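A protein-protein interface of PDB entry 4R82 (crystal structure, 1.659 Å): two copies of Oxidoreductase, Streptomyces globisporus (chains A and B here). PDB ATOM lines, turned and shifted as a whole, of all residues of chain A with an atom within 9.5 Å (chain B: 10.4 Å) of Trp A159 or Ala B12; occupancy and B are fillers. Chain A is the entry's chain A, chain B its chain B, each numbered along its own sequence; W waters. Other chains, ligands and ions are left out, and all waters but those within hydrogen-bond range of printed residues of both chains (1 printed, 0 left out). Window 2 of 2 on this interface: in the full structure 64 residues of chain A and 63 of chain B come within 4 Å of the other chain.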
ATOM      1  N   VAL A  84     -21.536   5.153 -22.963  1.00  0.00           N
ATOM      2  CA  VAL A  84     -20.200   4.610 -23.187  1.00  0.00           C
ATOM      3  C   VAL A  84     -20.316   3.352 -24.036  1.00  0.00           C
ATOM      4  O   VAL A  84     -21.071   2.438 -23.696  1.00  0.00           O
ATOM      5  CB  VAL A  84     -19.517   4.260 -21.842  1.00  0.00           C
ATOM      6  CG1 VAL A  84     -18.130   3.628 -22.080  1.00  0.00           C
ATOM      7  CG2 VAL A  84     -19.407   5.486 -20.952  1.00  0.00           C
ATOM      8  N   SER A  85     -19.559   3.291 -25.139  1.00  0.00           N
ATOM      9  CA  SER A  85     -19.517   2.093 -25.954  1.00  0.00           C
ATOM     10  C   SER A  85     -18.115   1.537 -25.828  1.00  0.00           C
ATOM     11  O   SER A  85     -17.151   2.181 -26.262  1.00  0.00           O
ATOM     12  CB  SER A  85     -19.825   2.415 -27.421  1.00  0.00           C
ATOM     13  OG  SER A  85     -21.135   2.944 -27.570  1.00  0.00           O
ATOM     14  N   VAL A  86     -17.998   0.353 -25.231  1.00  0.00           N
ATOM     15  CA  VAL A  86     -16.701  -0.293 -25.088  1.00  0.00           C
ATOM     16  C   VAL A  86     -16.364  -0.975 -26.402  1.00  0.00           C
ATOM     17  O   VAL A  86     -17.075  -1.887 -26.843  1.00  0.00           O
ATOM     18  CB  VAL A  86     -16.713  -1.335 -23.971  1.00  0.00           C
ATOM     19  CG1 VAL A  86     -15.374  -2.077 -23.919  1.00  0.00           C
ATOM     20  CG2 VAL A  86     -17.038  -0.672 -22.634  1.00  0.00           C
ATOM     21  N   GLU A  88     -14.908  -3.180 -29.397  1.00  0.00           N
ATOM     22  CA  GLU A  88     -14.500  -4.549 -29.625  1.00  0.00           C
ATOM     23  C   GLU A  88     -13.172  -4.608 -30.387  1.00  0.00           C
ATOM     24  O   GLU A  88     -12.763  -3.629 -31.008  1.00  0.00           O
ATOM     25  CB  GLU A  88     -15.638  -5.249 -30.387  1.00  0.00           C
ATOM     26  CG  GLU A  88     -15.474  -6.717 -30.661  1.00  0.00           C
ATOM     27  CD  GLU A  88     -14.738  -6.967 -31.961  1.00  0.00           C
ATOM     28  OE1 GLU A  88     -14.748  -6.054 -32.819  1.00  0.00           O
ATOM     29  OE2 GLU A  88     -14.145  -8.059 -32.117  1.00  0.00           O
ATOM     30  N   GLN A  91     -12.432  -2.858 -33.891  1.00  0.00           N
ATOM     31  CA  GLN A  91     -12.988  -1.526 -34.112  1.00  0.00           C
ATOM     32  C   GLN A  91     -11.976  -0.386 -34.050  1.00  0.00           C
ATOM     33  O   GLN A  91     -12.308   0.725 -33.623  1.00  0.00           O
ATOM     34  CB  GLN A  91     -14.127  -1.268 -33.133  1.00  0.00           C
ATOM     35  CG  GLN A  91     -15.290  -2.232 -33.327  1.00  0.00           C
ATOM     36  CD  GLN A  91     -16.494  -1.839 -32.511  1.00  0.00           C
ATOM     37  OE1 GLN A  91     -16.456  -1.865 -31.276  1.00  0.00           O
ATOM     38  NE2 GLN A  91     -17.567  -1.429 -33.194  1.00  0.00           N
ATOM     39  N   VAL A 116     -26.947   2.600 -32.920  1.00  0.00           N
ATOM     40  CA  VAL A 116     -28.344   2.464 -32.534  1.00  0.00           C
ATOM     41  C   VAL A 116     -28.622   3.513 -31.460  1.00  0.00           C
ATOM     42  O   VAL A 116     -27.736   3.857 -30.670  1.00  0.00           O
ATOM     43  CB  VAL A 116     -28.665   1.047 -31.987  1.00  0.00           C
ATOM     44  CG1 VAL A 116     -28.406  -0.009 -33.048  1.00  0.00           C
ATOM     45  CG2 VAL A 116     -27.852   0.742 -30.742  1.00  0.00           C
ATOM     46  N   LEU A 125     -25.339   4.768 -29.837  1.00  0.00           N
ATOM     47  CA  LEU A 125     -24.511   3.738 -29.225  1.00  0.00           C
ATOM     48  C   LEU A 125     -23.805   3.021 -30.372  1.00  0.00           C
ATOM     49  O   LEU A 125     -24.442   2.704 -31.369  1.00  0.00           O
ATOM     50  CB  LEU A 125     -25.389   2.740 -28.464  1.00  0.00           C
ATOM     51  CG  LEU A 125     -26.338   3.366 -27.443  1.00  0.00           C
ATOM     52  CD1 LEU A 125     -27.240   2.310 -26.825  1.00  0.00           C
ATOM     53  CD2 LEU A 125     -25.532   4.033 -26.378  1.00  0.00           C
ATOM     54  N   ILE A 126     -22.501   2.788 -30.253  1.00  0.00           N
ATOM     55  CA  ILE A 126     -21.744   2.274 -31.392  1.00  0.00           C
ATOM     56  C   ILE A 126     -22.013   0.785 -31.610  1.00  0.00           C
ATOM     57  O   ILE A 126     -21.810  -0.029 -30.705  1.00  0.00           O
ATOM     58  CB  ILE A 126     -20.230   2.507 -31.222  1.00  0.00           C
ATOM     59  CG1 ILE A 126     -19.941   3.976 -30.882  1.00  0.00           C
ATOM     60  CG2 ILE A 126     -19.482   2.105 -32.491  1.00  0.00           C
ATOM     61  CD1 ILE A 126     -20.513   4.979 -31.857  1.00  0.00           C
ATOM     62  N   ALA A 127     -22.482   0.429 -32.804  1.00  0.00           N
ATOM     63  CA  ALA A 127     -22.786  -0.969 -33.105  1.00  0.00           C
ATOM     64  C   ALA A 127     -21.493  -1.770 -33.108  1.00  0.00           C
ATOM     65  O   ALA A 127     -20.431  -1.240 -33.447  1.00  0.00           O
ATOM     66  CB  ALA A 127     -23.497  -1.085 -34.460  1.00  0.00           C
ATOM     67  N   GLY A 128     -21.573  -3.043 -32.725  1.00  0.00           N
ATOM     68  CA  GLY A 128     -20.393  -3.888 -32.714  1.00  0.00           C
ATOM     69  C   GLY A 128     -19.590  -3.839 -31.430  1.00  0.00           C
ATOM     70  O   GLY A 128     -18.606  -4.565 -31.287  1.00  0.00           O
ATOM     71  N   ALA A 129     -20.014  -2.997 -30.492  1.00  0.00           N
ATOM     72  CA  ALA A 129     -19.315  -2.816 -29.227  1.00  0.00           C
ATOM     73  C   ALA A 129     -19.446  -4.032 -28.308  1.00  0.00           C
ATOM     74  O   ALA A 129     -20.408  -4.806 -28.411  1.00  0.00           O
ATOM     75  CB  ALA A 129     -19.852  -1.575 -28.523  1.00  0.00           C
ATOM     76  N   VAL A 130     -18.498  -4.185 -27.385  1.00  0.00           N
ATOM     77  CA  VAL A 130     -18.573  -5.251 -26.391  1.00  0.00           C
ATOM     78  C   VAL A 130     -19.747  -4.975 -25.457  1.00  0.00           C
ATOM     79  O   VAL A 130     -20.471  -5.889 -25.035  1.00  0.00           O
ATOM     80  CB  VAL A 130     -17.264  -5.342 -25.573  1.00  0.00           C
ATOM     81  CG1 VAL A 130     -17.295  -6.540 -24.647  1.00  0.00           C
ATOM     82  CG2 VAL A 130     -16.078  -5.468 -26.508  1.00  0.00           C
ATOM     83  N   ALA A 131     -19.937  -3.697 -25.148  1.00  0.00           N
ATOM     84  CA  ALA A 131     -20.998  -3.296 -24.229  1.00  0.00           C
ATOM     85  C   ALA A 131     -21.398  -1.865 -24.443  1.00  0.00           C
ATOM     86  O   ALA A 131     -20.596  -1.055 -24.919  1.00  0.00           O
ATOM     87  CB  ALA A 131     -20.549  -3.494 -22.800  1.00  0.00           C
ATOM     88  N   HIS A 132     -22.638  -1.554 -24.056  1.00  0.00           N
ATOM     89  CA  HIS A 132     -23.133  -0.172 -24.018  1.00  0.00           C
ATOM     90  C   HIS A 132     -23.559   0.126 -22.593  1.00  0.00           C
ATOM     91  O   HIS A 132     -24.245  -0.690 -21.967  1.00  0.00           O
ATOM     92  CB  HIS A 132     -24.370  -0.016 -24.914  1.00  0.00           C
ATOM     93  CG  HIS A 132     -24.103  -0.197 -26.377  1.00  0.00           C
ATOM     94  ND1 HIS A 132     -25.070  -0.642 -27.251  1.00  0.00           N
ATOM     95  CD2 HIS A 132     -22.995   0.034 -27.124  1.00  0.00           C
ATOM     96  CE1 HIS A 132     -24.566  -0.694 -28.473  1.00  0.00           C
ATOM     97  NE2 HIS A 132     -23.308  -0.289 -28.423  1.00  0.00           N
ATOM     98  N   LEU A 133     -23.185   1.296 -22.082  1.00  0.00           N
ATOM     99  CA  LEU A 133     -23.661   1.733 -20.772  1.00  0.00           C
ATOM    100  C   LEU A 133     -24.257   3.108 -20.964  1.00  0.00           C
ATOM    101  O   LEU A 133     -23.649   3.961 -21.592  1.00  0.00           O
ATOM    102  CB  LEU A 133     -22.516   1.832 -19.762  1.00  0.00           C
ATOM    103  CG  LEU A 133     -21.703   0.584 -19.410  1.00  0.00           C
ATOM    104  CD1 LEU A 133     -20.555   0.380 -20.394  1.00  0.00           C
ATOM    105  CD2 LEU A 133     -21.190   0.652 -17.966  1.00  0.00           C
ATOM    106  N   GLU A 134     -25.460   3.319 -20.453  1.00  0.00           N
ATOM    107  CA  GLU A 134     -26.049   4.649 -20.466  1.00  0.00           C
ATOM    108  C   GLU A 134     -26.077   5.165 -19.039  1.00  0.00           C
ATOM    109  O   GLU A 134     -26.547   4.471 -18.126  1.00  0.00           O
ATOM    110  CB  GLU A 134     -27.446   4.605 -21.091  1.00  0.00           C
ATOM    111  CG  GLU A 134     -27.383   4.234 -22.576  1.00  0.00           C
ATOM    112  CD  GLU A 134     -28.745   4.083 -23.215  1.00  0.00           C
ATOM    113  OE1 GLU A 134     -29.356   5.117 -23.548  1.00  0.00           O
ATOM    114  OE2 GLU A 134     -29.190   2.929 -23.397  1.00  0.00           O
ATOM    115  N   ALA A 156     -27.496  -1.044 -19.095  1.00  0.00           N
ATOM    116  CA  ALA A 156     -26.352  -1.501 -19.863  1.00  0.00           C
ATOM    117  C   ALA A 156     -26.741  -2.744 -20.627  1.00  0.00           C
ATOM    118  O   ALA A 156     -27.667  -3.455 -20.225  1.00  0.00           O
ATOM    119  CB  ALA A 156     -25.150  -1.764 -18.955  1.00  0.00           C
ATOM    120  N   THR A 157     -26.056  -2.982 -21.744  1.00  0.00           N
ATOM    121  CA  THR A 157     -26.289  -4.180 -22.544  1.00  0.00           C
ATOM    122  C   THR A 157     -24.918  -4.692 -22.946  1.00  0.00           C
ATOM    123  O   THR A 157     -24.013  -3.892 -23.181  1.00  0.00           O
ATOM    124  CB  THR A 157     -27.113  -3.871 -23.804  1.00  0.00           C
ATOM    125  OG1 THR A 157     -28.445  -3.486 -23.426  1.00  0.00           O
ATOM    126  CG2 THR A 157     -27.198  -5.095 -24.701  1.00  0.00           C
ATOM    127  N   ARG A 158     -24.752  -6.010 -22.999  1.00  0.00           N
ATOM    128  CA  ARG A 158     -23.452  -6.555 -23.387  1.00  0.00           C
ATOM    129  C   ARG A 158     -23.606  -7.717 -24.366  1.00  0.00           C
ATOM    130  O   ARG A 158     -24.655  -8.352 -24.426  1.00  0.00           O
ATOM    131  CB  ARG A 158     -22.639  -6.961 -22.154  1.00  0.00           C
ATOM    132  CG  ARG A 158     -23.251  -8.078 -21.338  1.00  0.00           C
ATOM    133  CD  ARG A 158     -22.489  -8.284 -20.020  1.00  0.00           C
ATOM    134  NE  ARG A 158     -21.128  -8.764 -20.253  1.00  0.00           N
ATOM    135  CZ  ARG A 158     -20.776 -10.047 -20.282  1.00  0.00           C
ATOM    136  NH1 ARG A 158     -21.677 -11.004 -20.086  1.00  0.00           N
ATOM    137  NH2 ARG A 158     -19.509 -10.373 -20.508  1.00  0.00           N
ATOM    138  N   TRP A 159     -22.551  -7.958 -25.136  1.00  0.00           N
ATOM    139  CA  TRP A 159     -22.501  -9.038 -26.117  1.00  0.00           C
ATOM    140  C   TRP A 159     -21.366  -9.946 -25.695  1.00  0.00           C
ATOM    141  O   TRP A 159     -20.204  -9.687 -25.994  1.00  0.00           O
ATOM    142  CB  TRP A 159     -22.264  -8.475 -27.531  1.00  0.00           C
ATOM    143  CG  TRP A 159     -23.491  -7.820 -28.097  1.00  0.00           C
ATOM    144  CD1 TRP A 159     -24.391  -8.375 -28.965  1.00  0.00           C
ATOM    145  CD2 TRP A 159     -23.979  -6.503 -27.799  1.00  0.00           C
ATOM    146  NE1 TRP A 159     -25.399  -7.478 -29.238  1.00  0.00           N
ATOM    147  CE2 TRP A 159     -25.173  -6.323 -28.533  1.00  0.00           C
ATOM    148  CE3 TRP A 159     -23.519  -5.457 -26.992  1.00  0.00           C
ATOM    149  CZ2 TRP A 159     -25.917  -5.138 -28.481  1.00  0.00           C
ATOM    150  CZ3 TRP A 159     -24.267  -4.273 -26.934  1.00  0.00           C
ATOM    151  CH2 TRP A 159     -25.453  -4.128 -27.678  1.00  0.00           C
ATOM    152  N   PRO A 160     -21.699 -11.019 -24.976  1.00  0.00           N
ATOM    153  CA  PRO A 160     -20.673 -11.864 -24.357  1.00  0.00           C
ATOM    154  C   PRO A 160     -19.656 -12.458 -25.331  1.00  0.00           C
ATOM    155  O   PRO A 160     -18.537 -12.744 -24.916  1.00  0.00           O
ATOM    156  CB  PRO A 160     -21.490 -12.980 -23.708  1.00  0.00           C
ATOM    157  CG  PRO A 160     -22.814 -12.342 -23.421  1.00  0.00           C
ATOM    158  CD  PRO A 160     -23.062 -11.404 -24.571  1.00  0.00           C
ATOM    159  N   ALA A 161     -20.021 -12.639 -26.596  1.00  0.00           N
ATOM    160  CA  ALA A 161     -19.103 -13.269 -27.540  1.00  0.00           C
ATOM    161  C   ALA A 161     -17.967 -12.328 -27.930  1.00  0.00           C
ATOM    162  O   ALA A 161     -16.926 -12.774 -28.437  1.00  0.00           O
ATOM    163  CB  ALA A 161     -19.849 -13.758 -28.770  1.00  0.00           C
ATOM    164  N   ARG A 162     -18.169 -11.035 -27.693  1.00  0.00           N
ATOM    165  CA  ARG A 162     -17.194 -10.011 -28.095  1.00  0.00           C
ATOM    166  C   ARG A 162     -16.149  -9.737 -27.022  1.00  0.00           C
ATOM    167  O   ARG A 162     -16.419  -9.876 -25.826  1.00  0.00           O
ATOM    168  CB  ARG A 162     -17.906  -8.705 -28.459  1.00  0.00           C
ATOM    169  CG  ARG A 162     -18.835  -8.832 -29.672  1.00  0.00           C
ATOM    170  CD  ARG A 162     -19.643  -7.558 -29.907  1.00  0.00           C
ATOM    171  NE  ARG A 162     -20.540  -7.738 -31.050  1.00  0.00           N
ATOM    172  CZ  ARG A 162     -21.576  -6.956 -31.343  1.00  0.00           C
ATOM    173  NH1 ARG A 162     -22.309  -7.214 -32.422  1.00  0.00           N
ATOM    174  NH2 ARG A 162     -21.882  -5.924 -30.575  1.00  0.00           N
ATOM    175  N   GLU A 163     -14.968  -9.308 -27.463  1.00  0.00           N
ATOM    176  CA  GLU A 163     -13.868  -9.011 -26.558  1.00  0.00           C
ATOM    177  C   GLU A 163     -13.298  -7.643 -26.918  1.00  0.00           C
ATOM    178  O   GLU A 163     -13.228  -7.298 -28.097  1.00  0.00           O
ATOM    179  CB  GLU A 163     -12.806 -10.096 -26.752  1.00  0.00           C
ATOM    180  CG  GLU A 163     -11.626 -10.049 -25.827  1.00  0.00           C
ATOM    181  CD  GLU A 163     -10.962 -11.405 -25.737  1.00  0.00           C
ATOM    182  OE1 GLU A 163     -11.341 -12.185 -24.840  1.00  0.00           O
ATOM    183  OE2 GLU A 163     -10.091 -11.697 -26.581  1.00  0.00           O
ATOM    184  N   GLY A 164     -12.885  -6.862 -25.919  1.00  0.00           N
ATOM    185  CA  GLY A 164     -12.438  -5.495 -26.162  1.00  0.00           C
ATOM    186  C   GLY A 164     -11.097  -5.317 -26.870  1.00  0.00           C
ATOM    187  O   GLY A 164     -10.214  -6.177 -26.800  1.00  0.00           O
ATOM    188  N   ALA B  12     -27.931 -10.362 -27.298  1.00  0.00           N
ATOM    189  CA  ALA B  12     -27.389  -9.429 -26.311  1.00  0.00           C
ATOM    190  C   ALA B  12     -27.924  -9.715 -24.914  1.00  0.00           C
ATOM    191  O   ALA B  12     -29.055 -10.165 -24.759  1.00  0.00           O
ATOM    192  CB  ALA B  12     -27.709  -8.010 -26.707  1.00  0.00           C
ATOM    193  N   GLU B  13     -27.112  -9.444 -23.900  1.00  0.00           N
ATOM    194  CA  GLU B  13     -27.526  -9.636 -22.513  1.00  0.00           C
ATOM    195  C   GLU B  13     -27.890  -8.278 -21.922  1.00  0.00           C
ATOM    196  O   GLU B  13     -27.065  -7.368 -21.913  1.00  0.00           O
ATOM    197  CB  GLU B  13     -26.408 -10.293 -21.691  1.00  0.00           C
ATOM    198  CG  GLU B  13     -26.506 -10.062 -20.167  1.00  0.00           C
ATOM    199  CD  GLU B  13     -25.335 -10.659 -19.383  1.00  0.00           C
ATOM    200  OE1 GLU B  13     -24.441 -11.265 -20.007  1.00  0.00           O
ATOM    201  OE2 GLU B  13     -25.316 -10.530 -18.138  1.00  0.00           O
ATOM    202  N   LEU B  14     -29.123  -8.137 -21.446  1.00  0.00           N
ATOM    203  CA  LEU B  14     -29.534  -6.892 -20.802  1.00  0.00           C
ATOM    204  C   LEU B  14     -29.090  -6.945 -19.353  1.00  0.00           C
ATOM    205  O   LEU B  14     -29.334  -7.936 -18.668  1.00  0.00           O
ATOM    206  CB  LEU B  14     -31.055  -6.729 -20.874  1.00  0.00           C
ATOM    207  CG  LEU B  14     -31.628  -5.481 -20.193  1.00  0.00           C
ATOM    208  CD1 LEU B  14     -31.128  -4.193 -20.855  1.00  0.00           C
ATOM    209  CD2 LEU B  14     -33.157  -5.514 -20.163  1.00  0.00           C
ATOM    210  N   VAL B  15     -28.440  -5.883 -18.884  1.00  0.00           N
ATOM    211  CA  VAL B  15     -27.879  -5.839 -17.534  1.00  0.00           C
ATOM    212  C   VAL B  15     -28.755  -5.008 -16.605  1.00  0.00           C
ATOM    213  O   VAL B  15     -29.058  -3.855 -16.911  1.00  0.00           O
ATOM    214  CB  VAL B  15     -26.463  -5.229 -17.558  1.00  0.00           C
ATOM    215  CG1 VAL B  15     -25.968  -4.953 -16.143  1.00  0.00           C
ATOM    216  CG2 VAL B  15     -25.504  -6.157 -18.285  1.00  0.00           C
ATOM    217  N   ASP B  16     -29.188  -5.607 -15.494  1.00  0.00           N
ATOM    218  CA  ASP B  16     -29.893  -4.877 -14.436  1.00  0.00           C
ATOM    219  C   ASP B  16     -28.810  -4.304 -13.537  1.00  0.00           C
ATOM    220  O   ASP B  16     -28.050  -5.054 -12.921  1.00  0.00           O
ATOM    221  CB  ASP B  16     -30.810  -5.837 -13.662  1.00  0.00           C
ATOM    222  CG  ASP B  16     -31.443  -5.204 -12.417  1.00  0.00           C
ATOM    223  OD1 ASP B  16     -31.294  -3.980 -12.186  1.00  0.00           O
ATOM    224  OD2 ASP B  16     -32.105  -5.952 -11.663  1.00  0.00           O
ATOM    225  N   GLN B  22     -24.460  -9.222 -12.528  1.00  0.00           N
ATOM    226  CA  GLN B  22     -24.509  -8.670 -13.879  1.00  0.00           C
ATOM    227  C   GLN B  22     -23.655  -7.431 -14.047  1.00  0.00           C
ATOM    228  O   GLN B  22     -23.010  -7.246 -15.080  1.00  0.00           O
ATOM    229  CB  GLN B  22     -25.939  -8.316 -14.261  1.00  0.00           C
ATOM    230  CG  GLN B  22     -26.815  -9.505 -14.568  1.00  0.00           C
ATOM    231  CD  GLN B  22     -28.023  -9.063 -15.354  1.00  0.00           C
ATOM    232  OE1 GLN B  22     -28.852  -8.321 -14.847  1.00  0.00           O
ATOM    233  NE2 GLN B  22     -28.100  -9.472 -16.616  1.00  0.00           N
ATOM    234  N   ARG B  25     -20.165  -8.282 -14.470  1.00  0.00           N
ATOM    235  CA  ARG B  25     -19.932  -8.790 -15.819  1.00  0.00           C
ATOM    236  C   ARG B  25     -19.664  -7.650 -16.794  1.00  0.00           C
ATOM    237  O   ARG B  25     -18.717  -7.715 -17.588  1.00  0.00           O
ATOM    238  CB  ARG B  25     -21.109  -9.629 -16.314  1.00  0.00           C
ATOM    239  CG  ARG B  25     -21.165 -11.021 -15.745  1.00  0.00           C
ATOM    240  CD  ARG B  25     -22.289 -11.802 -16.401  1.00  0.00           C
ATOM    241  NE  ARG B  25     -22.643 -12.988 -15.636  1.00  0.00           N
ATOM    242  CZ  ARG B  25     -23.894 -13.364 -15.397  1.00  0.00           C
ATOM    243  NH1 ARG B  25     -24.901 -12.642 -15.871  1.00  0.00           N
ATOM    244  NH2 ARG B  25     -24.136 -14.458 -14.690  1.00  0.00           N
ATOM    245  N   VAL B  26     -20.478  -6.600 -16.739  1.00  0.00           N
ATOM    246  CA  VAL B  26     -20.271  -5.492 -17.670  1.00  0.00           C
ATOM    247  C   VAL B  26     -19.032  -4.664 -17.323  1.00  0.00           C
ATOM    248  O   VAL B  26     -18.334  -4.215 -18.225  1.00  0.00           O
ATOM    249  CB  VAL B  26     -21.549  -4.611 -17.894  1.00  0.00           C
ATOM    250  CG1 VAL B  26     -21.868  -3.776 -16.675  1.00  0.00           C
ATOM    251  CG2 VAL B  26     -21.365  -3.703 -19.110  1.00  0.00           C
ATOM    252  N   GLY B  28     -16.363  -5.879 -16.207  1.00  0.00           N
ATOM    253  CA  GLY B  28     -15.258  -6.710 -16.660  1.00  0.00           C
ATOM    254  C   GLY B  28     -15.085  -6.699 -18.172  1.00  0.00           C
ATOM    255  O   GLY B  28     -14.073  -7.188 -18.698  1.00  0.00           O
ATOM    256  N   ASP B  29     -16.070  -6.150 -18.884  1.00  0.00           N
ATOM    257  CA  ASP B  29     -15.973  -6.032 -20.344  1.00  0.00           C
ATOM    258  C   ASP B  29     -14.979  -4.971 -20.801  1.00  0.00           C
ATOM    259  O   ASP B  29     -14.557  -4.997 -21.954  1.00  0.00           O
ATOM    260  CB  ASP B  29     -17.337  -5.734 -20.973  1.00  0.00           C
ATOM    261  CG  ASP B  29     -18.219  -6.951 -21.041  1.00  0.00           C
ATOM    262  OD1 ASP B  29     -17.668  -8.078 -21.089  1.00  0.00           O
ATOM    263  OD2 ASP B  29     -19.454  -6.773 -21.062  1.00  0.00           O
ATOM    264  N   PHE B  30     -14.613  -4.044 -19.917  1.00  0.00           N
ATOM    265  CA  PHE B  30     -13.573  -3.059 -20.241  1.00  0.00           C
ATOM    266  C   PHE B  30     -12.233  -3.557 -19.723  1.00  0.00           C
ATOM    267  O   PHE B  30     -12.034  -3.679 -18.511  1.00  0.00           O
ATOM    268  CB  PHE B  30     -13.878  -1.716 -19.584  1.00  0.00           C
ATOM    269  CG  PHE B  30     -12.861  -0.645 -19.889  1.00  0.00           C
ATOM    270  CD1 PHE B  30     -12.858  -0.020 -21.130  1.00  0.00           C
ATOM    271  CD2 PHE B  30     -11.923  -0.256 -18.939  1.00  0.00           C
ATOM    272  CE1 PHE B  30     -11.937   0.984 -21.424  1.00  0.00           C
ATOM    273  CE2 PHE B  30     -10.984   0.761 -19.236  1.00  0.00           C
ATOM    274  CZ  PHE B  30     -11.002   1.372 -20.474  1.00  0.00           C
ATOM    275  N   GLY B 169     -12.784  -9.559 -18.146  1.00  0.00           N
ATOM    276  CA  GLY B 169     -13.764 -10.614 -17.914  1.00  0.00           C
ATOM    277  C   GLY B 169     -13.496 -11.399 -16.642  1.00  0.00           C
ATOM    278  O   GLY B 169     -13.838 -12.591 -16.559  1.00  0.00           O
HETATM  279  O   HOH W   1     -13.655  -7.206 -23.202  1.00  0.00           O
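No position is printed for both chains.
Of the 15 pairs that touch across the chains among the printed residues, none has its exchanged pair printed and touching as well.
Of the 12 printed residues of chain B, 7 touch a printed residue of chain A.
Among the printed residues, Asp or Glu carboxylates within 4 Å of a Lys or Arg side-chain nitrogen of the other chain: Arg A158 with Glu B13 (2.8 Å) and Arg A158 with Asp B29 (2.7 Å).
The backbone NH of Val A86 sits at hydrogen-bond distance from the backbone carbonyl oxygen of Ala A131 (3.0 Å).
O of Val A130 sits at hydrogen-bond distance from N of Trp A159 (2.9 Å).
N of His A132 lies within hydrogen-bond range of O of Thr A157, 2.8 Å away.
The side-chain carboxylate of Glu B13 lies within hydrogen-bond range of the side-chain amide nitrogen of Gln B22.
The guanidinium group (NH1) of Arg B25 is in salt-bridge range of the side-chain carboxylate (OE2) of Glu B13, 3.1 Å away.
NE2 of Gln B22 lies within hydrogen-bond range of O of Leu B14 (2.8 Å).
Ser A85 touches none of the printed residues of chain B.
Printed residues of chain B within 4 Å of Val A86: Asp B29.
Of chain B, only Asp B29 comes within 4 Å of Val A130.
His A132 touches none of the printed residues of chain B.
Thr A157 touches three residues of chain B.
Arg A158 touches just these residues of chain B: Ala B12 (3.5 Å), Glu B13 (2.7 Å), Arg B25 (3.7 Å) and Asp B29 (2.7 Å).
Printed residues of chain B within 4 Å of Trp A159: Ala B12.
No residue of chain B comes within 4 Å of Arg A162.
Of chain A, only Thr A157, Arg A158 and Trp A159 come within 4 Å of Ala B12.
Of the printed residues of chain A, Leu B14 touches Ala A156 and Thr A157.
Of the printed residues of chain A, Val B15 touches Ala A156 (2.9 Å).
Phe B30 touches none of the printed residues of chain A.
The backbone carbonyl oxygen (O) of Ala A156 lies within hydrogen-bond range of the backbone NH (N) of Val B15, at 2.9 Å.
The side-chain carboxylate of Glu B13 is in salt-bridge range of the guanidinium group of Arg A158 (2.8 Å).
The side-chain carboxylate (OD2) of Asp B29 is in salt-bridge range of the guanidinium group (NE) of Arg A158, at 2.7 Å.
Water W1 bridges O of Asp B29 (2.7 Å) and N of Gly A164 (2.8 Å).
Among the printed residues, merely in contact across the chains: Thr A157 with Glu B13 (3.3 Å), Trp A159 with Ala B12 (3.5 Å), Arg A158 with Ala B12 (3.5 Å), Thr A157 with Ala B12 (3.6 Å), Ala A156 with Leu B14 (3.6 Å), Val A86 with Asp B29 (3.6 Å), Arg A158 with Arg B25 (3.7 Å), Val A130 with Asp B29 (3.7 Å), Thr A157 with Leu B14 (3.8 Å), Ala A131 with Val B26 (3.8 Å), Ala A131 with Asp B29 (3.9 Å) and Pro A160 with Glu B13 (3.9 Å).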
